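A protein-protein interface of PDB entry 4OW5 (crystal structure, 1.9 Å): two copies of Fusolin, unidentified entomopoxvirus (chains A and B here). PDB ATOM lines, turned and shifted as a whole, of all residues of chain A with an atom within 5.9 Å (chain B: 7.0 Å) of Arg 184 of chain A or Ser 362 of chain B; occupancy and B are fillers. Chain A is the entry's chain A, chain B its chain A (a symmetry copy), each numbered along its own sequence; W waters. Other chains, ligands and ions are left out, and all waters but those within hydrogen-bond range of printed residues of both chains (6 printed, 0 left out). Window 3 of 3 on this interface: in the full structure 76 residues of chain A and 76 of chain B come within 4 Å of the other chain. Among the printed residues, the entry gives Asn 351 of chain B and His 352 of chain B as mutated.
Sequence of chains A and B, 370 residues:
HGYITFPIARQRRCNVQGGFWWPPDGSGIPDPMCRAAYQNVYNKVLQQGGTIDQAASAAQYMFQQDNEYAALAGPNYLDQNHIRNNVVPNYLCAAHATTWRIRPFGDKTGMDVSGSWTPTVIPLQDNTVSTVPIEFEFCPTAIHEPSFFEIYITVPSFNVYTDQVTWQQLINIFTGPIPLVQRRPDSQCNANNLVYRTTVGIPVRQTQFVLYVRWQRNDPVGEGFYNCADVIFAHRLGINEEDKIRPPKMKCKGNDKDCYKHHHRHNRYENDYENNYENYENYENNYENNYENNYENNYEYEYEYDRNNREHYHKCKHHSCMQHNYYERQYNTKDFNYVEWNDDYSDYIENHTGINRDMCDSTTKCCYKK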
ATOM      1  N   GLU A 135     -28.132 -13.008 -21.195  1.00  0.00           N
ATOM      2  CA  GLU A 135     -29.101 -12.563 -20.233  1.00  0.00           C
ATOM      3  C   GLU A 135     -28.689 -11.163 -19.747  1.00  0.00           C
ATOM      4  O   GLU A 135     -27.808 -11.025 -18.918  1.00  0.00           O
ATOM      5  CB  GLU A 135     -29.280 -13.546 -19.090  1.00  0.00           C
ATOM      6  CG  GLU A 135     -30.432 -13.148 -18.193  1.00  0.00           C
ATOM      7  CD  GLU A 135     -30.521 -13.962 -16.922  1.00  0.00           C
ATOM      8  OE1 GLU A 135     -29.542 -13.954 -16.138  1.00  0.00           O
ATOM      9  OE2 GLU A 135     -31.613 -14.508 -16.650  1.00  0.00           O
ATOM     10  N   GLU A 137     -28.679  -7.773 -17.734  1.00  0.00           N
ATOM     11  CA  GLU A 137     -28.955  -7.336 -16.366  1.00  0.00           C
ATOM     12  C   GLU A 137     -28.837  -5.824 -16.337  1.00  0.00           C
ATOM     13  O   GLU A 137     -27.797  -5.259 -16.722  1.00  0.00           O
ATOM     14  CB  GLU A 137     -28.016  -8.000 -15.326  1.00  0.00           C
ATOM     15  CG  GLU A 137     -28.482  -7.744 -13.904  1.00  0.00           C
ATOM     16  CD  GLU A 137     -27.530  -8.158 -12.799  1.00  0.00           C
ATOM     17  OE1 GLU A 137     -26.376  -7.678 -12.810  1.00  0.00           O
ATOM     18  OE2 GLU A 137     -27.958  -8.889 -11.876  1.00  0.00           O
ATOM     19  N   GLN A 182     -35.711 -10.510  -8.282  1.00  0.00           N
ATOM     20  CA  GLN A 182     -34.684 -10.498  -7.265  1.00  0.00           C
ATOM     21  C   GLN A 182     -33.358 -10.774  -7.920  1.00  0.00           C
ATOM     22  O   GLN A 182     -33.258 -11.668  -8.775  1.00  0.00           O
ATOM     23  CB  GLN A 182     -34.930 -11.532  -6.129  1.00  0.00           C
ATOM     24  CG  GLN A 182     -34.013 -11.315  -4.919  1.00  0.00           C
ATOM     25  CD  GLN A 182     -34.061 -12.474  -3.949  1.00  0.00           C
ATOM     26  OE1 GLN A 182     -35.105 -12.795  -3.387  1.00  0.00           O
ATOM     27  NE2 GLN A 182     -32.939 -13.153  -3.737  1.00  0.00           N
ATOM     28  N   ARG A 183     -32.337 -10.022  -7.511  1.00  0.00           N
ATOM     29  CA  ARG A 183     -30.991 -10.208  -8.022  1.00  0.00           C
ATOM     30  C   ARG A 183     -30.478 -11.578  -7.574  1.00  0.00           C
ATOM     31  O   ARG A 183     -30.799 -12.051  -6.469  1.00  0.00           O
ATOM     32  CB  ARG A 183     -30.035  -9.092  -7.519  1.00  0.00           C
ATOM     33  CG  ARG A 183     -29.535  -9.312  -6.092  1.00  0.00           C
ATOM     34  CD  ARG A 183     -28.690  -8.175  -5.511  1.00  0.00           C
ATOM     35  NE  ARG A 183     -27.256  -8.317  -5.756  1.00  0.00           N
ATOM     36  CZ  ARG A 183     -26.442  -9.194  -5.163  1.00  0.00           C
ATOM     37  NH1 ARG A 183     -26.916 -10.062  -4.270  1.00  0.00           N
ATOM     38  NH2 ARG A 183     -25.151  -9.224  -5.474  1.00  0.00           N
ATOM     39  N   ARG A 184     -29.682 -12.205  -8.402  1.00  0.00           N
ATOM     40  CA  ARG A 184     -29.112 -13.484  -8.026  1.00  0.00           C
ATOM     41  C   ARG A 184     -27.895 -13.265  -7.138  1.00  0.00           C
ATOM     42  O   ARG A 184     -27.302 -12.195  -7.182  1.00  0.00           O
ATOM     43  CB  ARG A 184     -28.699 -14.264  -9.256  1.00  0.00           C
ATOM     44  CG  ARG A 184     -29.829 -14.737 -10.137  1.00  0.00           C
ATOM     45  CD  ARG A 184     -29.340 -15.922 -10.939  1.00  0.00           C
ATOM     46  NE  ARG A 184     -30.267 -16.283 -12.009  1.00  0.00           N
ATOM     47  CZ  ARG A 184     -30.333 -15.677 -13.187  1.00  0.00           C
ATOM     48  NH1 ARG A 184     -29.536 -14.643 -13.460  1.00  0.00           N
ATOM     49  NH2 ARG A 184     -31.210 -16.075 -14.090  1.00  0.00           N
ATOM     50  N   PRO A 185     -27.454 -14.272  -6.362  1.00  0.00           N
ATOM     51  CA  PRO A 185     -26.243 -14.092  -5.525  1.00  0.00           C
ATOM     52  C   PRO A 185     -24.990 -13.653  -6.293  1.00  0.00           C
ATOM     53  O   PRO A 185     -24.166 -12.943  -5.730  1.00  0.00           O
ATOM     54  CB  PRO A 185     -26.043 -15.476  -4.910  1.00  0.00           C
ATOM     55  CG  PRO A 185     -27.452 -16.058  -4.865  1.00  0.00           C
ATOM     56  CD  PRO A 185     -28.079 -15.590  -6.141  1.00  0.00           C
ATOM     57  N   ASP A 186     -24.860 -14.017  -7.585  1.00  0.00           N
ATOM     58  CA  ASP A 186     -23.693 -13.614  -8.390  1.00  0.00           C
ATOM     59  C   ASP A 186     -23.908 -12.265  -9.147  1.00  0.00           C
ATOM     60  O   ASP A 186     -23.084 -11.895  -9.989  1.00  0.00           O
ATOM     61  CB  ASP A 186     -23.374 -14.715  -9.412  1.00  0.00           C
ATOM     62  CG  ASP A 186     -24.360 -14.858 -10.567  1.00  0.00           C
ATOM     63  OD1 ASP A 186     -25.508 -14.341 -10.455  1.00  0.00           O
ATOM     64  OD2 ASP A 186     -24.021 -15.540 -11.542  1.00  0.00           O
ATOM     65  N   SER A 187     -25.001 -11.546  -8.874  1.00  0.00           N
ATOM     66  CA  SER A 187     -25.280 -10.313  -9.581  1.00  0.00           C
ATOM     67  C   SER A 187     -24.148  -9.314  -9.550  1.00  0.00           C
ATOM     68  O   SER A 187     -23.448  -9.151  -8.552  1.00  0.00           O
ATOM     69  CB  SER A 187     -26.510  -9.634  -9.019  1.00  0.00           C
ATOM     70  OG  SER A 187     -26.686  -8.385  -9.672  1.00  0.00           O
ATOM     71  N   VAL A 195     -33.325  -6.266  -9.856  1.00  0.00           N
ATOM     72  CA  VAL A 195     -32.708  -5.968 -11.148  1.00  0.00           C
ATOM     73  C   VAL A 195     -33.745  -6.210 -12.233  1.00  0.00           C
ATOM     74  O   VAL A 195     -34.763  -6.867 -11.988  1.00  0.00           O
ATOM     75  CB  VAL A 195     -31.437  -6.829 -11.404  1.00  0.00           C
ATOM     76  CG1 VAL A 195     -30.293  -6.437 -10.470  1.00  0.00           C
ATOM     77  CG2 VAL A 195     -31.733  -8.325 -11.298  1.00  0.00           C
ATOM     78  N   ARG A 197     -33.915  -8.233 -15.660  1.00  0.00           N
ATOM     79  CA  ARG A 197     -33.205  -9.262 -16.433  1.00  0.00           C
ATOM     80  C   ARG A 197     -34.037  -9.809 -17.550  1.00  0.00           C
ATOM     81  O   ARG A 197     -35.196 -10.111 -17.338  1.00  0.00           O
ATOM     82  CB  ARG A 197     -32.797 -10.457 -15.593  1.00  0.00           C
ATOM     83  CG  ARG A 197     -31.716 -10.251 -14.615  1.00  0.00           C
ATOM     84  CD  ARG A 197     -31.172 -11.597 -14.140  1.00  0.00           C
ATOM     85  NE  ARG A 197     -32.187 -12.502 -13.588  1.00  0.00           N
ATOM     86  CZ  ARG A 197     -32.484 -12.664 -12.293  1.00  0.00           C
ATOM     87  NH1 ARG A 197     -31.849 -11.968 -11.364  1.00  0.00           N
ATOM     88  NH2 ARG A 197     -33.413 -13.536 -11.923  1.00  0.00           N
ATOM     89  N   TYR B 348     -19.265 -14.420 -14.717  1.00  0.00           N
ATOM     90  CA  TYR B 348     -20.617 -13.948 -15.053  1.00  0.00           C
ATOM     91  C   TYR B 348     -20.894 -14.167 -16.554  1.00  0.00           C
ATOM     92  O   TYR B 348     -21.939 -14.685 -16.920  1.00  0.00           O
ATOM     93  CB  TYR B 348     -20.828 -12.464 -14.688  1.00  0.00           C
ATOM     94  CG  TYR B 348     -22.296 -12.111 -14.515  1.00  0.00           C
ATOM     95  CD1 TYR B 348     -23.089 -11.782 -15.613  1.00  0.00           C
ATOM     96  CD2 TYR B 348     -22.920 -12.241 -13.280  1.00  0.00           C
ATOM     97  CE1 TYR B 348     -24.446 -11.534 -15.477  1.00  0.00           C
ATOM     98  CE2 TYR B 348     -24.289 -12.041 -13.139  1.00  0.00           C
ATOM     99  CZ  TYR B 348     -25.038 -11.619 -14.226  1.00  0.00           C
ATOM    100  OH  TYR B 348     -26.388 -11.409 -14.111  1.00  0.00           O
ATOM    101  N   ASN B 351     -21.519 -17.886 -17.213  1.00  0.00           N
ATOM    102  CA  ASN B 351     -22.774 -18.351 -16.653  1.00  0.00           C
ATOM    103  C   ASN B 351     -24.019 -17.703 -17.209  1.00  0.00           C
ATOM    104  O   ASN B 351     -25.093 -18.271 -16.997  1.00  0.00           O
ATOM    105  CB  ASN B 351     -22.770 -18.166 -15.128  1.00  0.00           C
ATOM    106  CG  ASN B 351     -21.740 -19.046 -14.471  1.00  0.00           C
ATOM    107  OD1 ASN B 351     -21.527 -20.188 -14.888  1.00  0.00           O
ATOM    108  ND2 ASN B 351     -21.064 -18.545 -13.446  1.00  0.00           N
ATOM    109  N   HIS B 352     -23.936 -16.521 -17.861  1.00  0.00           N
ATOM    110  CA  HIS B 352     -25.148 -15.819 -18.316  1.00  0.00           C
ATOM    111  C   HIS B 352     -25.143 -15.488 -19.802  1.00  0.00           C
ATOM    112  O   HIS B 352     -25.936 -14.657 -20.252  1.00  0.00           O
ATOM    113  CB  HIS B 352     -25.386 -14.572 -17.449  1.00  0.00           C
ATOM    114  CG  HIS B 352     -25.514 -14.954 -16.014  1.00  0.00           C
ATOM    115  ND1 HIS B 352     -26.645 -15.598 -15.546  1.00  0.00           N
ATOM    116  CD2 HIS B 352     -24.589 -14.934 -15.028  1.00  0.00           C
ATOM    117  CE1 HIS B 352     -26.406 -15.858 -14.267  1.00  0.00           C
ATOM    118  NE2 HIS B 352     -25.177 -15.494 -13.921  1.00  0.00           N
ATOM    119  N   ASP B 358     -27.243 -20.164 -16.812  1.00  0.00           N
ATOM    120  CA  ASP B 358     -28.068 -20.328 -15.620  1.00  0.00           C
ATOM    121  C   ASP B 358     -29.310 -19.517 -15.839  1.00  0.00           C
ATOM    122  O   ASP B 358     -29.195 -18.321 -16.037  1.00  0.00           O
ATOM    123  CB  ASP B 358     -27.328 -19.869 -14.355  1.00  0.00           C
ATOM    124  CG  ASP B 358     -28.225 -19.867 -13.114  1.00  0.00           C
ATOM    125  OD1 ASP B 358     -28.914 -20.886 -12.875  1.00  0.00           O
ATOM    126  OD2 ASP B 358     -28.289 -18.819 -12.428  1.00  0.00           O
ATOM    127  N   MET B 359     -30.479 -20.146 -15.862  1.00  0.00           N
ATOM    128  CA  MET B 359     -31.739 -19.450 -16.053  1.00  0.00           C
ATOM    129  C   MET B 359     -32.542 -19.509 -14.736  1.00  0.00           C
ATOM    130  O   MET B 359     -32.724 -18.491 -14.082  1.00  0.00           O
ATOM    131  CB  MET B 359     -32.530 -20.085 -17.207  1.00  0.00           C
ATOM    132  CG  MET B 359     -31.951 -19.885 -18.596  1.00  0.00           C
ATOM    133  SD  MET B 359     -32.772 -21.059 -19.764  1.00  0.00           S
ATOM    134  CE  MET B 359     -31.336 -21.994 -20.378  1.00  0.00           C
ATOM    135  N   CYS B 360     -32.969 -20.710 -14.345  1.00  0.00           N
ATOM    136  CA  CYS B 360     -33.822 -20.969 -13.200  1.00  0.00           C
ATOM    137  C   CYS B 360     -33.235 -21.920 -12.153  1.00  0.00           C
ATOM    138  O   CYS B 360     -33.726 -21.897 -11.035  1.00  0.00           O
ATOM    139  CB  CYS B 360     -35.132 -21.531 -13.728  1.00  0.00           C
ATOM    140  SG  CYS B 360     -36.055 -20.358 -14.739  1.00  0.00           S
ATOM    141  N   ASP B 361     -32.262 -22.779 -12.494  1.00  0.00           N
ATOM    142  CA  ASP B 361     -31.804 -23.813 -11.579  1.00  0.00           C
ATOM    143  C   ASP B 361     -31.184 -23.269 -10.293  1.00  0.00           C
ATOM    144  O   ASP B 361     -31.362 -23.890  -9.254  1.00  0.00           O
ATOM    145  CB  ASP B 361     -30.831 -24.776 -12.264  1.00  0.00           C
ATOM    146  CG  ASP B 361     -31.502 -25.737 -13.244  1.00  0.00           C
ATOM    147  OD1 ASP B 361     -32.756 -25.656 -13.414  1.00  0.00           O
ATOM    148  OD2 ASP B 361     -30.782 -26.561 -13.846  1.00  0.00           O
ATOM    149  N   SER B 362     -30.523 -22.116 -10.336  1.00  0.00           N
ATOM    150  CA  SER B 362     -29.932 -21.573  -9.106  1.00  0.00           C
ATOM    151  C   SER B 362     -30.968 -20.936  -8.186  1.00  0.00           C
ATOM    152  O   SER B 362     -30.630 -20.686  -7.040  1.00  0.00           O
ATOM    153  CB  SER B 362     -28.852 -20.541  -9.425  1.00  0.00           C
ATOM    154  OG  SER B 362     -29.407 -19.402 -10.051  1.00  0.00           O
ATOM    155  N   THR B 363     -32.190 -20.624  -8.677  1.00  0.00           N
ATOM    156  CA  THR B 363     -33.235 -19.954  -7.879  1.00  0.00           C
ATOM    157  C   THR B 363     -34.564 -20.722  -7.799  1.00  0.00           C
ATOM    158  O   THR B 363     -35.502 -20.216  -7.182  1.00  0.00           O
ATOM    159  CB  THR B 363     -33.536 -18.573  -8.505  1.00  0.00           C
ATOM    160  OG1 THR B 363     -34.314 -18.752  -9.694  1.00  0.00           O
ATOM    161  CG2 THR B 363     -32.262 -17.761  -8.818  1.00  0.00           C
ATOM    162  N   THR B 364     -34.679 -21.907  -8.441  1.00  0.00           N
ATOM    163  CA  THR B 364     -35.947 -22.646  -8.490  1.00  0.00           C
ATOM    164  C   THR B 364     -35.746 -24.105  -8.106  1.00  0.00           C
ATOM    165  O   THR B 364     -34.808 -24.741  -8.562  1.00  0.00           O
ATOM    166  CB  THR B 364     -36.546 -22.553  -9.912  1.00  0.00           C
ATOM    167  OG1 THR B 364     -36.481 -21.194 -10.361  1.00  0.00           O
ATOM    168  CG2 THR B 364     -37.985 -23.056  -9.985  1.00  0.00           C
ATOM    169  N   LYS B 365     -36.680 -24.651  -7.344  1.00  0.00           N
ATOM    170  CA  LYS B 365     -36.644 -26.051  -6.914  1.00  0.00           C
ATOM    171  C   LYS B 365     -37.964 -26.685  -7.286  1.00  0.00           C
ATOM    172  O   LYS B 365     -38.996 -26.027  -7.154  1.00  0.00           O
ATOM    173  CB  LYS B 365     -36.389 -26.145  -5.397  1.00  0.00           C
HETATM  174  O   HOH W   1     -21.558 -15.971 -12.218  1.00  0.00           O
HETATM  175  O   HOH W   2     -27.411 -13.113 -12.231  1.00  0.00           O
HETATM  176  O   HOH W   3     -27.841 -11.555 -16.340  1.00  0.00           O
HETATM  177  O   HOH W   4     -28.502 -16.391 -17.416  1.00  0.00           O
HETATM  178  O   HOH W   5     -26.200 -17.813 -11.198  1.00  0.00           O
HETATM  179  O   HOH W   6     -33.284 -17.279 -11.732  1.00  0.00           O
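Among the printed residues, merely in contact across the chains: Glu 137 of chain A with Tyr 348 of chain B (3.7 Å), Arg 184 of chain A with His 352 of chain B (3.5 Å), Arg 184 of chain A with Ser 362 of chain B (3.6 Å) and Asp 186 of chain A with Tyr 348 of chain B (3.3 Å).
No position is printed for both chains. Of the 8 pairs that touch across the chains among the printed residues, none has its exchanged pair printed and touching as well.
Of the 11 printed residues of chain B, 5 touch a printed residue of chain A. Hydrophobic or aromatic side chains of chain B within 4 Å of the printed part of chain A: Tyr 348 and His 352. Of the 10 printed residues of chain A, 4 touch a printed residue of chain B. Among the printed residues, 8 pairs touch across the chains. Among the printed residues, Asp or Glu carboxylates within 4 Å of a Lys or Arg side-chain nitrogen of the other chain: Arg 184 of chain A with Asp 358 of chain B.
Arg 184 of chain A touches just these residues of chain B: His 352 (3.5 Å), Asp 358 (3.2 Å), Met 359 (2.9 Å) and Ser 362 (3.6 Å). Of chain A, only Arg 184 comes within 4 Å of Ser 362 of chain B. Of the printed residues of chain A, Asp 358 of chain B touches Arg 184. Of the printed residues of chain A, Met 359 of chain B touches Arg 184. Arg 183 of chain A touches none of the printed residues of chain B. Thr 364 of chain B touches none of the printed residues of chain A. The nearest residue of chain B that does not touch Arg 184 of chain A is Thr 363 of chain B (4.04 Å).
OE2 of Glu 135 of chain A lies within salt-bridge range of NE of Arg 197 of chain A, 3.7 Å away. O of Asn 351 of chain B lies within hydrogen-bond range of N of Asp 358 of chain B (2.9 Å). The side-chain hydroxyl (OG) of Ser 187 of chain A sits at hydrogen-bond distance from the side-chain carboxylate (OE2) of Glu 137 of chain A, at 2.6 Å. The side-chain carboxylate (OE1) of Glu 135 of chain A lies within salt-bridge range of the guanidinium group (NH1) of Arg 184 of chain A, at 2.8 Å. The side-chain carboxylate (OD2) of Asp 358 of chain B is in hydrogen-bond range of the side-chain hydroxyl (OG) of Ser 362 of chain B, 2.7 Å away.
The backbone carbonyl oxygen (O) of His 352 of chain B is in hydrogen-bond range of the backbone NH (N) of Glu 135 of chain A, 2.9 Å away. OD2 of Asp 358 of chain B lies within salt-bridge range of NE of Arg 184 of chain A, 3.2 Å away. The side-chain carboxylate (OD2) of Asp 186 of chain A is in hydrogen-bond range of a ring nitrogen (NE2) of His 352 of chain B (2.6 Å). The backbone carbonyl oxygen (O) of Met 359 of chain B lies within hydrogen-bond range of the guanidinium group (NH2) of Arg 184 of chain A (2.9 Å).
Water W4 lies within hydrogen-bond range of O of Asp 358 of chain B, ND1 of His 352 of chain B and OE1 of Glu 135 of chain A. Water W1 bridges OD2 of Asp 186 of chain A (2.6 Å) and ND2 of Asn 351 of chain B (2.9 Å). Water W5 lies within hydrogen-bond range of OD2 of Asp 358 of chain B (2.6 Å) and OD2 of Asp 186 of chain A (3.2 Å). Water W3 lies within hydrogen-bond range of O of Glu 135 of chain A and OH of Tyr 348 of chain B. Water W6 lies within hydrogen-bond range of the backbone carbonyl oxygen of Met 359 of chain B (2.7 Å), the side-chain hydroxyl of Thr 363 of chain B (2.7 Å) and the guanidinium group of Arg 184 of chain A (3.2 Å). Water W2 lies within hydrogen-bond range of the side-chain hydroxyl (OH) of Tyr 348 of chain B (2.7 Å), the side-chain carboxylate (OD1) of Asp 186 of chain A (2.9 Å) and the guanidinium group (NH1) of Arg 184 of chain A (2.9 Å).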
